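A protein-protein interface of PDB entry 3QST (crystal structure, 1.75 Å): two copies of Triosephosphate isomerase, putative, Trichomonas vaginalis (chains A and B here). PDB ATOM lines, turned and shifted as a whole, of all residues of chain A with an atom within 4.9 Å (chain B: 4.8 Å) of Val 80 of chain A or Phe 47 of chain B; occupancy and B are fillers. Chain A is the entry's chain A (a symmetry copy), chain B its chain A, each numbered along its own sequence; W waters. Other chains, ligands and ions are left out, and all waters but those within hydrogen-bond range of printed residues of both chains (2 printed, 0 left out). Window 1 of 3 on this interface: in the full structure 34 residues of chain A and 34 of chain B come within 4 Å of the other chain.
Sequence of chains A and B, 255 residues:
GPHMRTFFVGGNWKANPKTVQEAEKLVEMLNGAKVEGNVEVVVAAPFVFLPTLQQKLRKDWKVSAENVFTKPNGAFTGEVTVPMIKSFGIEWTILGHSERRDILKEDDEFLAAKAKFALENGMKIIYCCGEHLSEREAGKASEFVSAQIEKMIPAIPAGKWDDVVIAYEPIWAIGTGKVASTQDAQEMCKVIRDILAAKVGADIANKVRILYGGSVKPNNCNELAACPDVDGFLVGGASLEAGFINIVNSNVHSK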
ATOM      1  N   PHE A  47      10.551 -17.431  20.935  1.00  0.00           N
ATOM      2  CA  PHE A  47      10.574 -18.230  19.715  1.00  0.00           C
ATOM      3  C   PHE A  47       9.181 -18.515  19.173  1.00  0.00           C
ATOM      4  O   PHE A  47       8.971 -18.461  17.963  1.00  0.00           O
ATOM      5  CB  PHE A  47      11.250 -19.588  19.935  1.00  0.00           C
ATOM      6  CG  PHE A  47      12.728 -19.513  20.189  1.00  0.00           C
ATOM      7  CD1 PHE A  47      13.582 -18.975  19.241  1.00  0.00           C
ATOM      8  CD2 PHE A  47      13.261 -20.024  21.374  1.00  0.00           C
ATOM      9  CE1 PHE A  47      14.959 -18.919  19.467  1.00  0.00           C
ATOM     10  CE2 PHE A  47      14.630 -19.991  21.609  1.00  0.00           C
ATOM     11  CZ  PHE A  47      15.485 -19.432  20.655  1.00  0.00           C
ATOM     12  N   VAL A  48       8.250 -18.865  20.061  1.00  0.00           N
ATOM     13  CA  VAL A  48       6.934 -19.318  19.598  1.00  0.00           C
ATOM     14  C   VAL A  48       6.092 -18.204  18.997  1.00  0.00           C
ATOM     15  O   VAL A  48       5.094 -18.472  18.310  1.00  0.00           O
ATOM     16  CB  VAL A  48       6.125 -20.059  20.684  1.00  0.00           C
ATOM     17  CG1 VAL A  48       6.794 -21.397  21.011  1.00  0.00           C
ATOM     18  CG2 VAL A  48       5.910 -19.175  21.936  1.00  0.00           C
ATOM     19  N   VAL A  68      20.066 -18.217  19.763  1.00  0.00           N
ATOM     20  CA  VAL A  68      20.118 -19.366  18.851  1.00  0.00           C
ATOM     21  C   VAL A  68      21.212 -20.293  19.341  1.00  0.00           C
ATOM     22  O   VAL A  68      22.073 -19.872  20.118  1.00  0.00           O
ATOM     23  CB  VAL A  68      20.469 -18.967  17.391  1.00  0.00           C
ATOM     24  CG1 VAL A  68      19.326 -18.172  16.739  1.00  0.00           C
ATOM     25  CG2 VAL A  68      21.800 -18.205  17.328  1.00  0.00           C
ATOM     26  N   PHE A  69      21.205 -21.535  18.855  1.00  0.00           N
ATOM     27  CA  PHE A  69      22.236 -22.504  19.220  1.00  0.00           C
ATOM     28  C   PHE A  69      23.456 -22.367  18.292  1.00  0.00           C
ATOM     29  O   PHE A  69      23.514 -21.480  17.432  1.00  0.00           O
ATOM     30  CB  PHE A  69      21.630 -23.932  19.222  1.00  0.00           C
ATOM     31  CG  PHE A  69      22.507 -24.985  19.861  1.00  0.00           C
ATOM     32  CD1 PHE A  69      22.933 -24.869  21.192  1.00  0.00           C
ATOM     33  CD2 PHE A  69      22.874 -26.116  19.137  1.00  0.00           C
ATOM     34  CE1 PHE A  69      23.735 -25.851  21.769  1.00  0.00           C
ATOM     35  CE2 PHE A  69      23.685 -27.094  19.698  1.00  0.00           C
ATOM     36  CZ  PHE A  69      24.115 -26.968  21.019  1.00  0.00           C
ATOM     37  N   GLY A  78      15.298 -29.085  22.685  1.00  0.00           N
ATOM     38  CA  GLY A  78      14.959 -27.792  23.254  1.00  0.00           C
ATOM     39  C   GLY A  78      15.552 -26.591  22.524  1.00  0.00           C
ATOM     40  O   GLY A  78      15.071 -25.474  22.713  1.00  0.00           O
ATOM     41  N   GLU A  79      16.585 -26.809  21.709  1.00  0.00           N
ATOM     42  CA  GLU A  79      17.293 -25.700  21.055  1.00  0.00           C
ATOM     43  C   GLU A  79      16.702 -25.293  19.708  1.00  0.00           C
ATOM     44  O   GLU A  79      16.233 -26.135  18.945  1.00  0.00           O
ATOM     45  CB  GLU A  79      18.776 -26.032  20.860  1.00  0.00           C
ATOM     46  CG  GLU A  79      19.550 -26.146  22.172  1.00  0.00           C
ATOM     47  CD  GLU A  79      19.473 -24.879  23.001  1.00  0.00           C
ATOM     48  OE1 GLU A  79      19.887 -23.815  22.492  1.00  0.00           O
ATOM     49  OE2 GLU A  79      18.989 -24.937  24.154  1.00  0.00           O
ATOM     50  N   VAL A  80      16.755 -23.997  19.414  1.00  0.00           N
ATOM     51  CA  VAL A  80      16.391 -23.487  18.087  1.00  0.00           C
ATOM     52  C   VAL A  80      17.640 -23.042  17.330  1.00  0.00           C
ATOM     53  O   VAL A  80      18.550 -22.456  17.917  1.00  0.00           O
ATOM     54  CB  VAL A  80      15.406 -22.296  18.201  1.00  0.00           C
ATOM     55  CG1 VAL A  80      15.168 -21.626  16.838  1.00  0.00           C
ATOM     56  CG2 VAL A  80      14.077 -22.760  18.816  1.00  0.00           C
ATOM     57  N   THR A  81      17.699 -23.340  16.035  1.00  0.00           N
ATOM     58  CA  THR A  81      18.918 -23.074  15.269  1.00  0.00           C
ATOM     59  C   THR A  81      18.718 -21.992  14.211  1.00  0.00           C
ATOM     60  O   THR A  81      17.593 -21.643  13.859  1.00  0.00           O
ATOM     61  CB  THR A  81      19.449 -24.352  14.603  1.00  0.00           C
ATOM     62  OG1 THR A  81      18.523 -24.766  13.600  1.00  0.00           O
ATOM     63  CG2 THR A  81      19.623 -25.480  15.647  1.00  0.00           C
ATOM     64  N   VAL A  82      19.832 -21.457  13.727  1.00  0.00           N
ATOM     65  CA  VAL A  82      19.831 -20.410  12.706  1.00  0.00           C
ATOM     66  C   VAL A  82      19.026 -20.775  11.451  1.00  0.00           C
ATOM     67  O   VAL A  82      18.204 -19.975  10.987  1.00  0.00           O
ATOM     68  CB  VAL A  82      21.288 -19.999  12.351  1.00  0.00           C
ATOM     69  CG1 VAL A  82      21.340 -19.155  11.085  1.00  0.00           C
ATOM     70  CG2 VAL A  82      21.912 -19.248  13.525  1.00  0.00           C
ATOM     71  N   MET A  84      16.522 -22.605  11.146  1.00  0.00           N
ATOM     72  CA  MET A  84      15.089 -22.634  11.443  1.00  0.00           C
ATOM     73  C   MET A  84      14.516 -21.218  11.408  1.00  0.00           C
ATOM     74  O   MET A  84      13.462 -20.971  10.827  1.00  0.00           O
ATOM     75  CB  MET A  84      14.833 -23.239  12.825  1.00  0.00           C
ATOM     76  CG  MET A  84      15.306 -24.679  12.989  1.00  0.00           C
ATOM     77  SD  MET A  84      15.026 -25.160  14.705  1.00  0.00           S
ATOM     78  CE  MET A  84      15.865 -26.744  14.797  1.00  0.00           C
ATOM     79  N   ILE A  85      15.203 -20.306  12.088  1.00  0.00           N
ATOM     80  CA  ILE A  85      14.866 -18.889  12.075  1.00  0.00           C
ATOM     81  C   ILE A  85      14.851 -18.309  10.651  1.00  0.00           C
ATOM     82  O   ILE A  85      13.899 -17.615  10.248  1.00  0.00           O
ATOM     83  CB  ILE A  85      15.898 -18.106  12.937  1.00  0.00           C
ATOM     84  CG1 ILE A  85      15.848 -18.616  14.376  1.00  0.00           C
ATOM     85  CG2 ILE A  85      15.630 -16.618  12.902  1.00  0.00           C
ATOM     86  CD1 ILE A  85      14.487 -18.565  14.945  1.00  0.00           C
ATOM     87  N   ALA B  45       8.524 -30.808  18.747  1.00  0.00           N
ATOM     88  CA  ALA B  45       9.271 -30.120  17.697  1.00  0.00           C
ATOM     89  C   ALA B  45       9.876 -28.838  18.248  1.00  0.00           C
ATOM     90  O   ALA B  45       9.482 -28.397  19.318  1.00  0.00           O
ATOM     91  CB  ALA B  45       8.332 -29.798  16.525  1.00  0.00           C
ATOM     92  N   PRO B  46      10.829 -28.232  17.513  1.00  0.00           N
ATOM     93  CA  PRO B  46      11.428 -26.951  17.907  1.00  0.00           C
ATOM     94  C   PRO B  46      10.396 -25.844  18.096  1.00  0.00           C
ATOM     95  O   PRO B  46       9.392 -25.829  17.386  1.00  0.00           O
ATOM     96  CB  PRO B  46      12.341 -26.619  16.725  1.00  0.00           C
ATOM     97  CG  PRO B  46      12.731 -27.957  16.167  1.00  0.00           C
ATOM     98  CD  PRO B  46      11.465 -28.785  16.301  1.00  0.00           C
ATOM     99  N   PHE B  47      10.644 -24.928  19.032  1.00  0.00           N
ATOM    100  CA  PHE B  47       9.650 -23.922  19.388  1.00  0.00           C
ATOM    101  C   PHE B  47       9.067 -23.215  18.173  1.00  0.00           C
ATOM    102  O   PHE B  47       7.864 -22.967  18.127  1.00  0.00           O
ATOM    103  CB  PHE B  47      10.238 -22.833  20.294  1.00  0.00           C
ATOM    104  CG  PHE B  47      10.600 -23.302  21.674  1.00  0.00           C
ATOM    105  CD1 PHE B  47       9.633 -23.815  22.521  1.00  0.00           C
ATOM    106  CD2 PHE B  47      11.914 -23.184  22.131  1.00  0.00           C
ATOM    107  CE1 PHE B  47       9.961 -24.235  23.812  1.00  0.00           C
ATOM    108  CE2 PHE B  47      12.256 -23.583  23.418  1.00  0.00           C
ATOM    109  CZ  PHE B  47      11.278 -24.115  24.262  1.00  0.00           C
ATOM    110  N   VAL B  48       9.925 -22.850  17.221  1.00  0.00           N
ATOM    111  CA  VAL B  48       9.464 -22.018  16.104  1.00  0.00           C
ATOM    112  C   VAL B  48       8.547 -22.756  15.143  1.00  0.00           C
ATOM    113  O   VAL B  48       7.856 -22.128  14.326  1.00  0.00           O
ATOM    114  CB  VAL B  48      10.615 -21.350  15.323  1.00  0.00           C
ATOM    115  CG1 VAL B  48      11.303 -20.301  16.202  1.00  0.00           C
ATOM    116  CG2 VAL B  48      11.604 -22.398  14.758  1.00  0.00           C
ATOM    117  N   PHE B  49       8.525 -24.084  15.255  1.00  0.00           N
ATOM    118  CA  PHE B  49       7.655 -24.906  14.422  1.00  0.00           C
ATOM    119  C   PHE B  49       6.375 -25.316  15.149  1.00  0.00           C
ATOM    120  O   PHE B  49       5.501 -25.947  14.554  1.00  0.00           O
ATOM    121  CB  PHE B  49       8.373 -26.184  13.949  1.00  0.00           C
ATOM    122  CG  PHE B  49       9.614 -25.936  13.126  1.00  0.00           C
ATOM    123  CD1 PHE B  49       9.772 -24.762  12.390  1.00  0.00           C
ATOM    124  CD2 PHE B  49      10.626 -26.893  13.081  1.00  0.00           C
ATOM    125  CE1 PHE B  49      10.924 -24.549  11.647  1.00  0.00           C
ATOM    126  CE2 PHE B  49      11.780 -26.683  12.329  1.00  0.00           C
ATOM    127  CZ  PHE B  49      11.924 -25.512  11.608  1.00  0.00           C
ATOM    128  N   LEU B  50       6.267 -24.979  16.432  1.00  0.00           N
ATOM    129  CA  LEU B  50       5.121 -25.424  17.209  1.00  0.00           C
ATOM    130  C   LEU B  50       3.804 -24.829  16.687  1.00  0.00           C
ATOM    131  O   LEU B  50       2.799 -25.529  16.605  1.00  0.00           O
ATOM    132  CB  LEU B  50       5.314 -25.139  18.706  1.00  0.00           C
ATOM    133  CG  LEU B  50       6.405 -25.948  19.434  1.00  0.00           C
ATOM    134  CD1 LEU B  50       6.490 -25.487  20.878  1.00  0.00           C
ATOM    135  CD2 LEU B  50       6.132 -27.472  19.373  1.00  0.00           C
ATOM    136  N   PRO B  51       3.809 -23.541  16.307  1.00  0.00           N
ATOM    137  CA  PRO B  51       2.526 -23.044  15.807  1.00  0.00           C
ATOM    138  C   PRO B  51       2.045 -23.775  14.561  1.00  0.00           C
ATOM    139  O   PRO B  51       0.855 -24.099  14.450  1.00  0.00           O
ATOM    140  CB  PRO B  51       2.813 -21.559  15.532  1.00  0.00           C
ATOM    141  CG  PRO B  51       3.899 -21.229  16.525  1.00  0.00           C
ATOM    142  CD  PRO B  51       4.784 -22.445  16.508  1.00  0.00           C
ATOM    143  N   ALA B  65       6.034 -29.320  23.306  1.00  0.00           N
ATOM    144  CA  ALA B  65       7.282 -28.555  23.315  1.00  0.00           C
ATOM    145  C   ALA B  65       8.399 -29.501  23.726  1.00  0.00           C
ATOM    146  O   ALA B  65       8.135 -30.581  24.278  1.00  0.00           O
ATOM    147  CB  ALA B  65       7.199 -27.398  24.300  1.00  0.00           C
ATOM    148  N   ASN B  67      10.921 -28.369  25.750  1.00  0.00           N
ATOM    149  CA  ASN B  67      11.437 -27.765  26.981  1.00  0.00           C
ATOM    150  C   ASN B  67      10.548 -26.565  27.310  1.00  0.00           C
ATOM    151  O   ASN B  67       9.876 -26.043  26.424  1.00  0.00           O
ATOM    152  CB  ASN B  67      12.874 -27.263  26.778  1.00  0.00           C
ATOM    153  CG  ASN B  67      13.470 -26.655  28.051  1.00  0.00           C
ATOM    154  OD1 ASN B  67      13.317 -27.207  29.145  1.00  0.00           O
ATOM    155  ND2 ASN B  67      14.149 -25.512  27.908  1.00  0.00           N
ATOM    156  N   VAL B  80      11.251 -19.815  26.608  1.00  0.00           N
ATOM    157  CA  VAL B  80       9.815 -19.941  26.336  1.00  0.00           C
ATOM    158  C   VAL B  80       9.090 -20.498  27.558  1.00  0.00           C
ATOM    159  O   VAL B  80       9.603 -21.388  28.236  1.00  0.00           O
ATOM    160  CB  VAL B  80       9.560 -20.868  25.119  1.00  0.00           C
ATOM    161  CG1 VAL B  80       8.063 -21.168  24.940  1.00  0.00           C
ATOM    162  CG2 VAL B  80      10.146 -20.245  23.842  1.00  0.00           C
ATOM    163  N   ILE B  85       3.159 -21.449  25.361  1.00  0.00           N
ATOM    164  CA  ILE B  85       2.787 -22.714  24.743  1.00  0.00           C
ATOM    165  C   ILE B  85       1.272 -22.968  24.807  1.00  0.00           C
ATOM    166  O   ILE B  85       0.635 -23.322  23.797  1.00  0.00           O
ATOM    167  CB  ILE B  85       3.532 -23.876  25.461  1.00  0.00           C
ATOM    168  CG1 ILE B  85       5.040 -23.677  25.318  1.00  0.00           C
ATOM    169  CG2 ILE B  85       3.128 -25.221  24.899  1.00  0.00           C
ATOM    170  CD1 ILE B  85       5.457 -23.527  23.911  1.00  0.00           C
HETATM  171  O   HOH W   1      12.683 -26.076  20.981  1.00  0.00           O
HETATM  172  O   HOH W   2      14.837 -24.162  25.317  1.00  0.00           O
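O of Val 80 of chain A sits at hydrogen-bond distance from N of Phe 69 of chain A (3.0 Å).
The backbone NH of Thr 81 of chain A sits at hydrogen-bond distance from the side-chain sulfur of Met 84 of chain A (3.5 Å).
CB of Phe 47 of chain A touches CB of Phe 47 of chain B, at 3.4 Å.
Val 48 of chain B touches Phe 47 of chain A.
Val 48 of chain A touches Phe 47 of chain B (CG1 to O, 3.5 Å).
Val 48 of chain A touches Pro 51 of chain B (O to CG, 3.5 Å).
Gly 78 of chain A touches Phe 47 of chain B.
Phe 47 of chain B touches Val 80 of chain A.
Met 84 of chain A touches Pro 46 of chain B.
Met 84 of chain A touches Val 48 of chain B.
Met 84 of chain A touches Phe 49 of chain B (CG to CZ, 3.7 Å).
CD1 of Ile 85 of chain A touches CG1 of Val 48 of chain B (3.8 Å).
Phe 69 of chain A touches none of the printed residues of chain B.
Of the printed residues of chain B, Gly 78 of chain A touches Phe 47 (3.5 Å).
Of the printed residues of chain B, Val 80 of chain A touches Phe 47.
Printed residues of chain A within 4 Å of Pro 46 of chain B: Met 84.
Of the printed residues of chain A, Phe 47 of chain B touches Phe 47, Val 48, Gly 78 and Val 80.
The nearest printed residue of chain B that does not touch Val 80 of chain A is Val 48 of chain B (4.1 Å).
The nearest printed residue of chain A that does not touch Phe 47 of chain B is Glu 79 of chain A (5.7 Å).
The nearest printed residue of chain A that does not touch Pro 51 of chain B is Phe 47 of chain A (6.0 Å).
Hydrophobic or aromatic side chains of chain B that line the printed part of chain A: Pro 46, Phe 47, Val 48, Phe 49, Pro 51, Val 80 and Ile 85.
Of the 11 printed residues of chain A, 6 touch a printed residue of chain B.
Hydrophobic or aromatic side chains of chain A within 4 Å of the printed part of chain B: Phe 47, Val 48, Val 80, Met 84 and Ile 85.
Among the printed residues, 12 pairs touch across the chains.
Among the printed residues, no Asp or Glu carboxylate lies within 4 Å of a Lys or Arg side-chain nitrogen of the other chain.
Phe 47 of chain A touches its own counterpart, Phe 47 of chain B.
Phe 47 of chain A touches Val 48 of chain B, and with the chains exchanged Val 48 of chain A touches Phe 47 of chain B.
Phe 47 of chain A touches Val 80 of chain B, and with the chains exchanged Val 80 of chain A touches Phe 47 of chain B.
Val 48 of chain A touches Ile 85 of chain B, and with the chains exchanged Ile 85 of chain A touches Val 48 of chain B.
Water W2 lies within hydrogen-bond range of the backbone carbonyl oxygen (O) of Gly 78 of chain A (2.9 Å) and the side-chain amide nitrogen (ND2) of Asn 67 of chain B (3.0 Å).
Water W1 lies within hydrogen-bond range of the backbone carbonyl oxygen of Gly 78 of chain A (3.0 Å) and the backbone NH of Phe 47 of chain B (3.0 Å).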
